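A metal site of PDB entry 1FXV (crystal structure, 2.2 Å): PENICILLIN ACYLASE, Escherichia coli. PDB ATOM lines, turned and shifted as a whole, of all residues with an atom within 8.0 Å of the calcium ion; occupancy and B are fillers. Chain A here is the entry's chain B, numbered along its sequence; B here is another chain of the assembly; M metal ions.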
ATOM      1  N   GLY A  72      -5.853 -27.691   1.221  1.00  0.00           N
ATOM      2  CA  GLY A  72      -5.419 -27.624  -0.161  1.00  0.00           C
ATOM      3  C   GLY A  72      -5.295 -26.147  -0.505  1.00  0.00           C
ATOM      4  O   GLY A  72      -5.722 -25.291   0.278  1.00  0.00           O
ATOM      5  N   ASP A  73      -4.726 -25.833  -1.661  1.00  0.00           N
ATOM      6  CA  ASP A  73      -4.628 -24.435  -2.071  1.00  0.00           C
ATOM      7  C   ASP A  73      -5.798 -24.102  -2.996  1.00  0.00           C
ATOM      8  O   ASP A  73      -5.751 -24.365  -4.201  1.00  0.00           O
ATOM      9  CB  ASP A  73      -3.321 -24.167  -2.806  1.00  0.00           C
ATOM     10  CG  ASP A  73      -3.123 -22.697  -3.141  1.00  0.00           C
ATOM     11  OD1 ASP A  73      -4.090 -21.920  -2.968  1.00  0.00           O
ATOM     12  OD2 ASP A  73      -2.017 -22.315  -3.561  1.00  0.00           O
ATOM     13  N   ASP A  74      -6.850 -23.526  -2.418  1.00  0.00           N
ATOM     14  CA  ASP A  74      -8.036 -23.196  -3.184  1.00  0.00           C
ATOM     15  C   ASP A  74      -8.252 -21.682  -3.265  1.00  0.00           C
ATOM     16  O   ASP A  74      -9.301 -21.217  -3.731  1.00  0.00           O
ATOM     17  CB  ASP A  74      -9.275 -23.899  -2.583  1.00  0.00           C
ATOM     18  CG  ASP A  74      -9.520 -23.535  -1.117  1.00  0.00           C
ATOM     19  OD1 ASP A  74      -8.635 -22.919  -0.497  1.00  0.00           O
ATOM     20  OD2 ASP A  74     -10.599 -23.866  -0.579  1.00  0.00           O
ATOM     21  N   VAL A  75      -7.247 -20.930  -2.836  1.00  0.00           N
ATOM     22  CA  VAL A  75      -7.292 -19.465  -2.848  1.00  0.00           C
ATOM     23  C   VAL A  75      -6.067 -18.847  -3.527  1.00  0.00           C
ATOM     24  O   VAL A  75      -4.928 -19.089  -3.106  1.00  0.00           O
ATOM     25  CB  VAL A  75      -7.357 -18.910  -1.406  1.00  0.00           C
ATOM     26  CG1 VAL A  75      -7.564 -17.401  -1.439  1.00  0.00           C
ATOM     27  CG2 VAL A  75      -8.463 -19.593  -0.625  1.00  0.00           C
ATOM     28  N   ASP A  76      -6.285 -18.045  -4.567  1.00  0.00           N
ATOM     29  CA  ASP A  76      -5.199 -17.314  -5.217  1.00  0.00           C
ATOM     30  C   ASP A  76      -5.447 -15.797  -5.174  1.00  0.00           C
ATOM     31  O   ASP A  76      -6.588 -15.348  -5.148  1.00  0.00           O
ATOM     32  CB  ASP A  76      -5.043 -17.729  -6.679  1.00  0.00           C
ATOM     33  CG  ASP A  76      -4.503 -19.142  -6.843  1.00  0.00           C
ATOM     34  OD1 ASP A  76      -3.815 -19.627  -5.923  1.00  0.00           O
ATOM     35  OD2 ASP A  76      -4.745 -19.743  -7.912  1.00  0.00           O
ATOM     36  N   ILE A  77      -4.368 -15.021  -5.189  1.00  0.00           N
ATOM     37  CA  ILE A  77      -4.472 -13.566  -5.169  1.00  0.00           C
ATOM     38  C   ILE A  77      -4.204 -12.985  -6.556  1.00  0.00           C
ATOM     39  O   ILE A  77      -3.170 -13.242  -7.171  1.00  0.00           O
ATOM     40  CB  ILE A  77      -3.455 -12.951  -4.170  1.00  0.00           C
ATOM     41  CG1 ILE A  77      -3.746 -13.440  -2.747  1.00  0.00           C
ATOM     42  CG2 ILE A  77      -3.492 -11.438  -4.259  1.00  0.00           C
ATOM     43  CD1 ILE A  77      -5.146 -13.103  -2.241  1.00  0.00           C
ATOM     44  N   SER A 140      -9.187 -14.589  -4.645  1.00  0.00           N
ATOM     45  CA  SER A 140      -9.988 -15.476  -5.471  1.00  0.00           C
ATOM     46  C   SER A 140     -10.100 -16.884  -4.888  1.00  0.00           C
ATOM     47  O   SER A 140      -9.126 -17.639  -4.862  1.00  0.00           O
ATOM     48  CB  SER A 140      -9.387 -15.536  -6.881  1.00  0.00           C
ATOM     49  OG  SER A 140     -10.131 -16.410  -7.718  1.00  0.00           O
ATOM     50  N   PRO A 197      -8.874 -24.745  -8.488  1.00  0.00           N
ATOM     51  CA  PRO A 197      -8.705 -24.078  -9.782  1.00  0.00           C
ATOM     52  C   PRO A 197      -7.834 -24.802 -10.797  1.00  0.00           C
ATOM     53  O   PRO A 197      -6.847 -25.465 -10.462  1.00  0.00           O
ATOM     54  CB  PRO A 197      -8.132 -22.719  -9.380  1.00  0.00           C
ATOM     55  CG  PRO A 197      -7.284 -23.068  -8.189  1.00  0.00           C
ATOM     56  CD  PRO A 197      -8.196 -24.011  -7.414  1.00  0.00           C
ATOM     57  N   ARG A 199      -5.402 -23.891 -13.131  1.00  0.00           N
ATOM     58  CA  ARG A 199      -4.558 -22.718 -13.338  1.00  0.00           C
ATOM     59  C   ARG A 199      -3.865 -22.725 -14.706  1.00  0.00           C
ATOM     60  O   ARG A 199      -3.616 -23.790 -15.278  1.00  0.00           O
ATOM     61  CB  ARG A 199      -3.499 -22.633 -12.235  1.00  0.00           C
ATOM     62  CG  ARG A 199      -4.082 -22.656 -10.817  1.00  0.00           C
ATOM     63  CD  ARG A 199      -3.016 -22.340  -9.777  1.00  0.00           C
ATOM     64  NE  ARG A 199      -3.549 -22.074  -8.443  1.00  0.00           N
ATOM     65  CZ  ARG A 199      -3.886 -23.016  -7.551  1.00  0.00           C
ATOM     66  NH1 ARG A 199      -3.743 -24.297  -7.845  1.00  0.00           N
ATOM     67  NH2 ARG A 199      -4.319 -22.652  -6.356  1.00  0.00           N
ATOM     68  N   HIS A 203       1.592 -20.881 -13.846  1.00  0.00           N
ATOM     69  CA  HIS A 203       1.064 -20.162 -12.688  1.00  0.00           C
ATOM     70  C   HIS A 203       1.560 -20.824 -11.396  1.00  0.00           C
ATOM     71  O   HIS A 203       1.171 -21.947 -11.072  1.00  0.00           O
ATOM     72  CB  HIS A 203      -0.476 -20.162 -12.743  1.00  0.00           C
ATOM     73  CG  HIS A 203      -1.133 -19.542 -11.545  1.00  0.00           C
ATOM     74  ND1 HIS A 203      -2.452 -19.150 -11.561  1.00  0.00           N
ATOM     75  CD2 HIS A 203      -0.677 -19.290 -10.295  1.00  0.00           C
ATOM     76  CE1 HIS A 203      -2.779 -18.672 -10.375  1.00  0.00           C
ATOM     77  NE2 HIS A 203      -1.718 -18.738  -9.587  1.00  0.00           N
ATOM     78  N   ASP A 204       2.416 -20.118 -10.669  1.00  0.00           N
ATOM     79  CA  ASP A 204       2.911 -20.583  -9.372  1.00  0.00           C
ATOM     80  C   ASP A 204       1.834 -20.234  -8.339  1.00  0.00           C
ATOM     81  O   ASP A 204       1.620 -19.058  -8.039  1.00  0.00           O
ATOM     82  CB  ASP A 204       4.220 -19.849  -9.007  1.00  0.00           C
ATOM     83  CG  ASP A 204       4.930 -20.473  -7.814  1.00  0.00           C
ATOM     84  OD1 ASP A 204       4.268 -20.799  -6.816  1.00  0.00           O
ATOM     85  OD2 ASP A 204       6.166 -20.617  -7.884  1.00  0.00           O
ATOM     86  N   PRO A 205       1.144 -21.243  -7.793  1.00  0.00           N
ATOM     87  CA  PRO A 205       0.060 -21.039  -6.817  1.00  0.00           C
ATOM     88  C   PRO A 205       0.489 -20.455  -5.478  1.00  0.00           C
ATOM     89  O   PRO A 205      -0.342 -20.178  -4.630  1.00  0.00           O
ATOM     90  CB  PRO A 205      -0.535 -22.442  -6.670  1.00  0.00           C
ATOM     91  CG  PRO A 205       0.679 -23.326  -6.842  1.00  0.00           C
ATOM     92  CD  PRO A 205       1.363 -22.681  -8.027  1.00  0.00           C
ATOM     93  N   ARG A 206       1.799 -20.275  -5.292  1.00  0.00           N
ATOM     94  CA  ARG A 206       2.330 -19.713  -4.048  1.00  0.00           C
ATOM     95  C   ARG A 206       2.462 -18.193  -4.124  1.00  0.00           C
ATOM     96  O   ARG A 206       2.639 -17.529  -3.110  1.00  0.00           O
ATOM     97  CB  ARG A 206       3.706 -20.306  -3.744  1.00  0.00           C
ATOM     98  CG  ARG A 206       3.727 -21.800  -3.532  1.00  0.00           C
ATOM     99  CD  ARG A 206       5.161 -22.302  -3.494  1.00  0.00           C
ATOM    100  NE  ARG A 206       5.876 -22.020  -4.738  1.00  0.00           N
ATOM    101  CZ  ARG A 206       7.131 -22.360  -4.972  1.00  0.00           C
ATOM    102  NH1 ARG A 206       7.832 -22.998  -4.051  1.00  0.00           N
ATOM    103  NH2 ARG A 206       7.705 -22.058  -6.135  1.00  0.00           N
ATOM    104  N   LEU A 207       2.391 -17.643  -5.328  1.00  0.00           N
ATOM    105  CA  LEU A 207       2.597 -16.210  -5.513  1.00  0.00           C
ATOM    106  C   LEU A 207       1.455 -15.562  -6.295  1.00  0.00           C
ATOM    107  O   LEU A 207       0.761 -16.220  -7.056  1.00  0.00           O
ATOM    108  CB  LEU A 207       3.925 -15.980  -6.244  1.00  0.00           C
ATOM    109  CG  LEU A 207       5.150 -16.617  -5.582  1.00  0.00           C
ATOM    110  CD1 LEU A 207       6.382 -16.362  -6.432  1.00  0.00           C
ATOM    111  CD2 LEU A 207       5.329 -16.036  -4.191  1.00  0.00           C
ATOM    112  N   PRO A 208       1.242 -14.249  -6.097  1.00  0.00           N
ATOM    113  CA  PRO A 208       0.173 -13.527  -6.799  1.00  0.00           C
ATOM    114  C   PRO A 208       0.301 -13.610  -8.314  1.00  0.00           C
ATOM    115  O   PRO A 208       1.385 -13.874  -8.832  1.00  0.00           O
ATOM    116  CB  PRO A 208       0.335 -12.092  -6.304  1.00  0.00           C
ATOM    117  CG  PRO A 208       0.872 -12.272  -4.921  1.00  0.00           C
ATOM    118  CD  PRO A 208       1.910 -13.372  -5.114  1.00  0.00           C
ATOM    119  N   TRP A 217      -8.077 -18.107 -14.087  1.00  0.00           N
ATOM    120  CA  TRP A 217      -8.173 -19.556 -14.061  1.00  0.00           C
ATOM    121  C   TRP A 217      -8.902 -20.049 -15.307  1.00  0.00           C
ATOM    122  O   TRP A 217      -9.804 -19.376 -15.821  1.00  0.00           O
ATOM    123  CB  TRP A 217      -8.935 -20.026 -12.815  1.00  0.00           C
ATOM    124  CG  TRP A 217      -8.273 -19.679 -11.504  1.00  0.00           C
ATOM    125  CD1 TRP A 217      -6.947 -19.444 -11.295  1.00  0.00           C
ATOM    126  CD2 TRP A 217      -8.893 -19.630 -10.213  1.00  0.00           C
ATOM    127  NE1 TRP A 217      -6.701 -19.259  -9.954  1.00  0.00           N
ATOM    128  CE2 TRP A 217      -7.880 -19.369  -9.270  1.00  0.00           C
ATOM    129  CE3 TRP A 217     -10.211 -19.794  -9.758  1.00  0.00           C
ATOM    130  CZ2 TRP A 217      -8.132 -19.270  -7.899  1.00  0.00           C
ATOM    131  CZ3 TRP A 217     -10.472 -19.693  -8.398  1.00  0.00           C
ATOM    132  CH2 TRP A 217      -9.437 -19.431  -7.484  1.00  0.00           C
ATOM    133  N   ALA A 250       0.108 -28.436  -0.981  1.00  0.00           N
ATOM    134  CA  ALA A 250      -0.557 -27.865   0.188  1.00  0.00           C
ATOM    135  C   ALA A 250      -0.928 -26.399   0.008  1.00  0.00           C
ATOM    136  O   ALA A 250      -0.530 -25.746  -0.958  1.00  0.00           O
ATOM    137  CB  ALA A 250       0.339 -28.000   1.409  1.00  0.00           C
ATOM    138  N   SER A 251      -1.701 -25.904   0.965  1.00  0.00           N
ATOM    139  CA  SER A 251      -2.056 -24.493   1.048  1.00  0.00           C
ATOM    140  C   SER A 251      -0.806 -23.627   0.857  1.00  0.00           C
ATOM    141  O   SER A 251       0.306 -24.044   1.197  1.00  0.00           O
ATOM    142  CB  SER A 251      -2.682 -24.200   2.413  1.00  0.00           C
ATOM    143  OG  SER A 251      -2.831 -22.817   2.614  1.00  0.00           O
ATOM    144  N   ASP A 252      -0.980 -22.415   0.314  1.00  0.00           N
ATOM    145  CA  ASP A 252       0.164 -21.547   0.066  1.00  0.00           C
ATOM    146  C   ASP A 252       0.680 -20.808   1.295  1.00  0.00           C
ATOM    147  O   ASP A 252       1.691 -20.108   1.223  1.00  0.00           O
ATOM    148  CB  ASP A 252      -0.126 -20.532  -1.066  1.00  0.00           C
ATOM    149  CG  ASP A 252      -1.284 -19.591  -0.752  1.00  0.00           C
ATOM    150  OD1 ASP A 252      -1.325 -19.030   0.363  1.00  0.00           O
ATOM    151  OD2 ASP A 252      -2.134 -19.381  -1.639  1.00  0.00           O
ATOM    152  N   LEU A 253      -0.001 -20.978   2.431  1.00  0.00           N
ATOM    153  CA  LEU A 253       0.421 -20.363   3.696  1.00  0.00           C
ATOM    154  C   LEU A 253       1.886 -20.677   3.996  1.00  0.00           C
ATOM    155  O   LEU A 253       2.255 -21.829   4.115  1.00  0.00           O
ATOM    156  CB  LEU A 253      -0.428 -20.894   4.856  1.00  0.00           C
ATOM    157  CG  LEU A 253      -1.885 -20.497   4.907  1.00  0.00           C
ATOM    158  CD1 LEU A 253      -2.559 -21.215   6.061  1.00  0.00           C
ATOM    159  CD2 LEU A 253      -2.015 -18.983   5.064  1.00  0.00           C
ATOM    160  N   SER B 149      -7.696 -19.584   3.244  1.00  0.00           N
ATOM    161  CA  SER B 149      -6.322 -19.330   3.642  1.00  0.00           C
ATOM    162  C   SER B 149      -5.377 -19.029   2.483  1.00  0.00           C
ATOM    163  O   SER B 149      -5.305 -19.786   1.507  1.00  0.00           O
ATOM    164  CB  SER B 149      -5.771 -20.525   4.423  1.00  0.00           C
ATOM    165  OG  SER B 149      -6.508 -20.741   5.612  1.00  0.00           O
ATOM    166  N   THR B 150      -4.635 -17.930   2.602  1.00  0.00           N
ATOM    167  CA  THR B 150      -3.603 -17.595   1.638  1.00  0.00           C
ATOM    168  C   THR B 150      -2.645 -16.551   2.207  1.00  0.00           C
ATOM    169  O   THR B 150      -3.060 -15.655   2.929  1.00  0.00           O
ATOM    170  CB  THR B 150      -4.199 -17.051   0.321  1.00  0.00           C
ATOM    171  OG1 THR B 150      -3.160 -16.908  -0.654  1.00  0.00           O
ATOM    172  CG2 THR B 150      -4.859 -15.705   0.552  1.00  0.00           C
ATOM    173  N   SER B 151      -1.363 -16.679   1.869  1.00  0.00           N
ATOM    174  CA  SER B 151      -0.344 -15.714   2.303  1.00  0.00           C
ATOM    175  C   SER B 151       0.543 -15.330   1.122  1.00  0.00           C
ATOM    176  O   SER B 151       1.703 -14.968   1.300  1.00  0.00           O
ATOM    177  CB  SER B 151       0.518 -16.313   3.421  1.00  0.00           C
ATOM    178  OG  SER B 151       1.301 -17.396   2.950  1.00  0.00           O
ATOM    179  N   GLU B 152      -0.028 -15.392  -0.079  1.00  0.00           N
ATOM    180  CA  GLU B 152       0.702 -15.136  -1.313  1.00  0.00           C
ATOM    181  C   GLU B 152       1.433 -13.794  -1.352  1.00  0.00           C
ATOM    182  O   GLU B 152       2.533 -13.697  -1.891  1.00  0.00           O
ATOM    183  CB  GLU B 152      -0.237 -15.221  -2.503  1.00  0.00           C
ATOM    184  CG  GLU B 152      -0.512 -16.613  -2.995  1.00  0.00           C
ATOM    185  CD  GLU B 152      -1.430 -16.605  -4.210  1.00  0.00           C
ATOM    186  OE1 GLU B 152      -1.493 -15.537  -4.875  1.00  0.00           O
ATOM    187  OE2 GLU B 152      -2.074 -17.644  -4.494  1.00  0.00           O
ATOM    188  N   ASN B 155       4.357 -14.267   0.810  1.00  0.00           N
ATOM    189  CA  ASN B 155       5.213 -15.205   0.097  1.00  0.00           C
ATOM    190  C   ASN B 155       6.067 -14.487  -0.960  1.00  0.00           C
ATOM    191  O   ASN B 155       7.277 -14.705  -1.028  1.00  0.00           O
ATOM    192  CB  ASN B 155       4.373 -16.289  -0.584  1.00  0.00           C
ATOM    193  CG  ASN B 155       3.593 -17.141   0.413  1.00  0.00           C
ATOM    194  OD1 ASN B 155       2.766 -17.958   0.024  1.00  0.00           O
ATOM    195  ND2 ASN B 155       3.858 -16.965   1.707  1.00  0.00           N
HETATM  196 CA    CA M   1      -2.634 -19.798  -3.939  1.00  0.00          CA
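N of Ser 151 of chain B lies within hydrogen-bond range of OD1 of Asp 252, 2.8 Å away.
The backbone NH of Ile 77 lies within hydrogen-bond range of the side-chain carboxylate of Glu 152 of chain B, at 2.9 Å.
OG1 of Thr 150 of chain B sits close to OD1 of Asp 252, at 3.0 Å.
OD2 of Asp 76 is in salt-bridge range of NE of Arg 199 (2.7 Å).
The backbone carbonyl oxygen (O) of Asp 76 sits at hydrogen-bond distance from the backbone NH (N) of Ser 140 (2.8 Å).
The backbone carbonyl oxygen (O) of Asp 73 sits at hydrogen-bond distance from the guanidinium group (NH2) of Arg 199 (3.1 Å).
The backbone carbonyl oxygen (O) of Asp 252 sits close to the side-chain amide oxygen (OD1) of Asn 155 of chain B, 2.7 Å away.
NE1 of Trp 217 is in hydrogen-bond range of OD2 of Asp 76, at 2.9 Å.
Along chain A the residues within 4 Å of the calcium ion span positions 73 to 252.
The nearest printed residue that does not touch the calcium ion is Arg 199 (4.1 Å).
OE2 of Glu 152 of chain B is bound to the calcium ion (2.3 Å).
The calcium ion is bound by the side-chain carboxylate (OD1) of Asp 76 (2.3 Å).
The calcium ion is bound by OD2 of Asp 252 (2.4 Å).
The backbone carbonyl oxygen (O) of Pro 205 is bound to the calcium ion.
O of Val 75 binds the calcium ion, 2.5 Å away.
The calcium ion is bound by the side-chain carboxylate (OD2) of Asp 73 (2.6 Å).
The calcium ion is bound by OD1 of Asp 73.
The calcium ion has seven donor atoms within binding distance.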
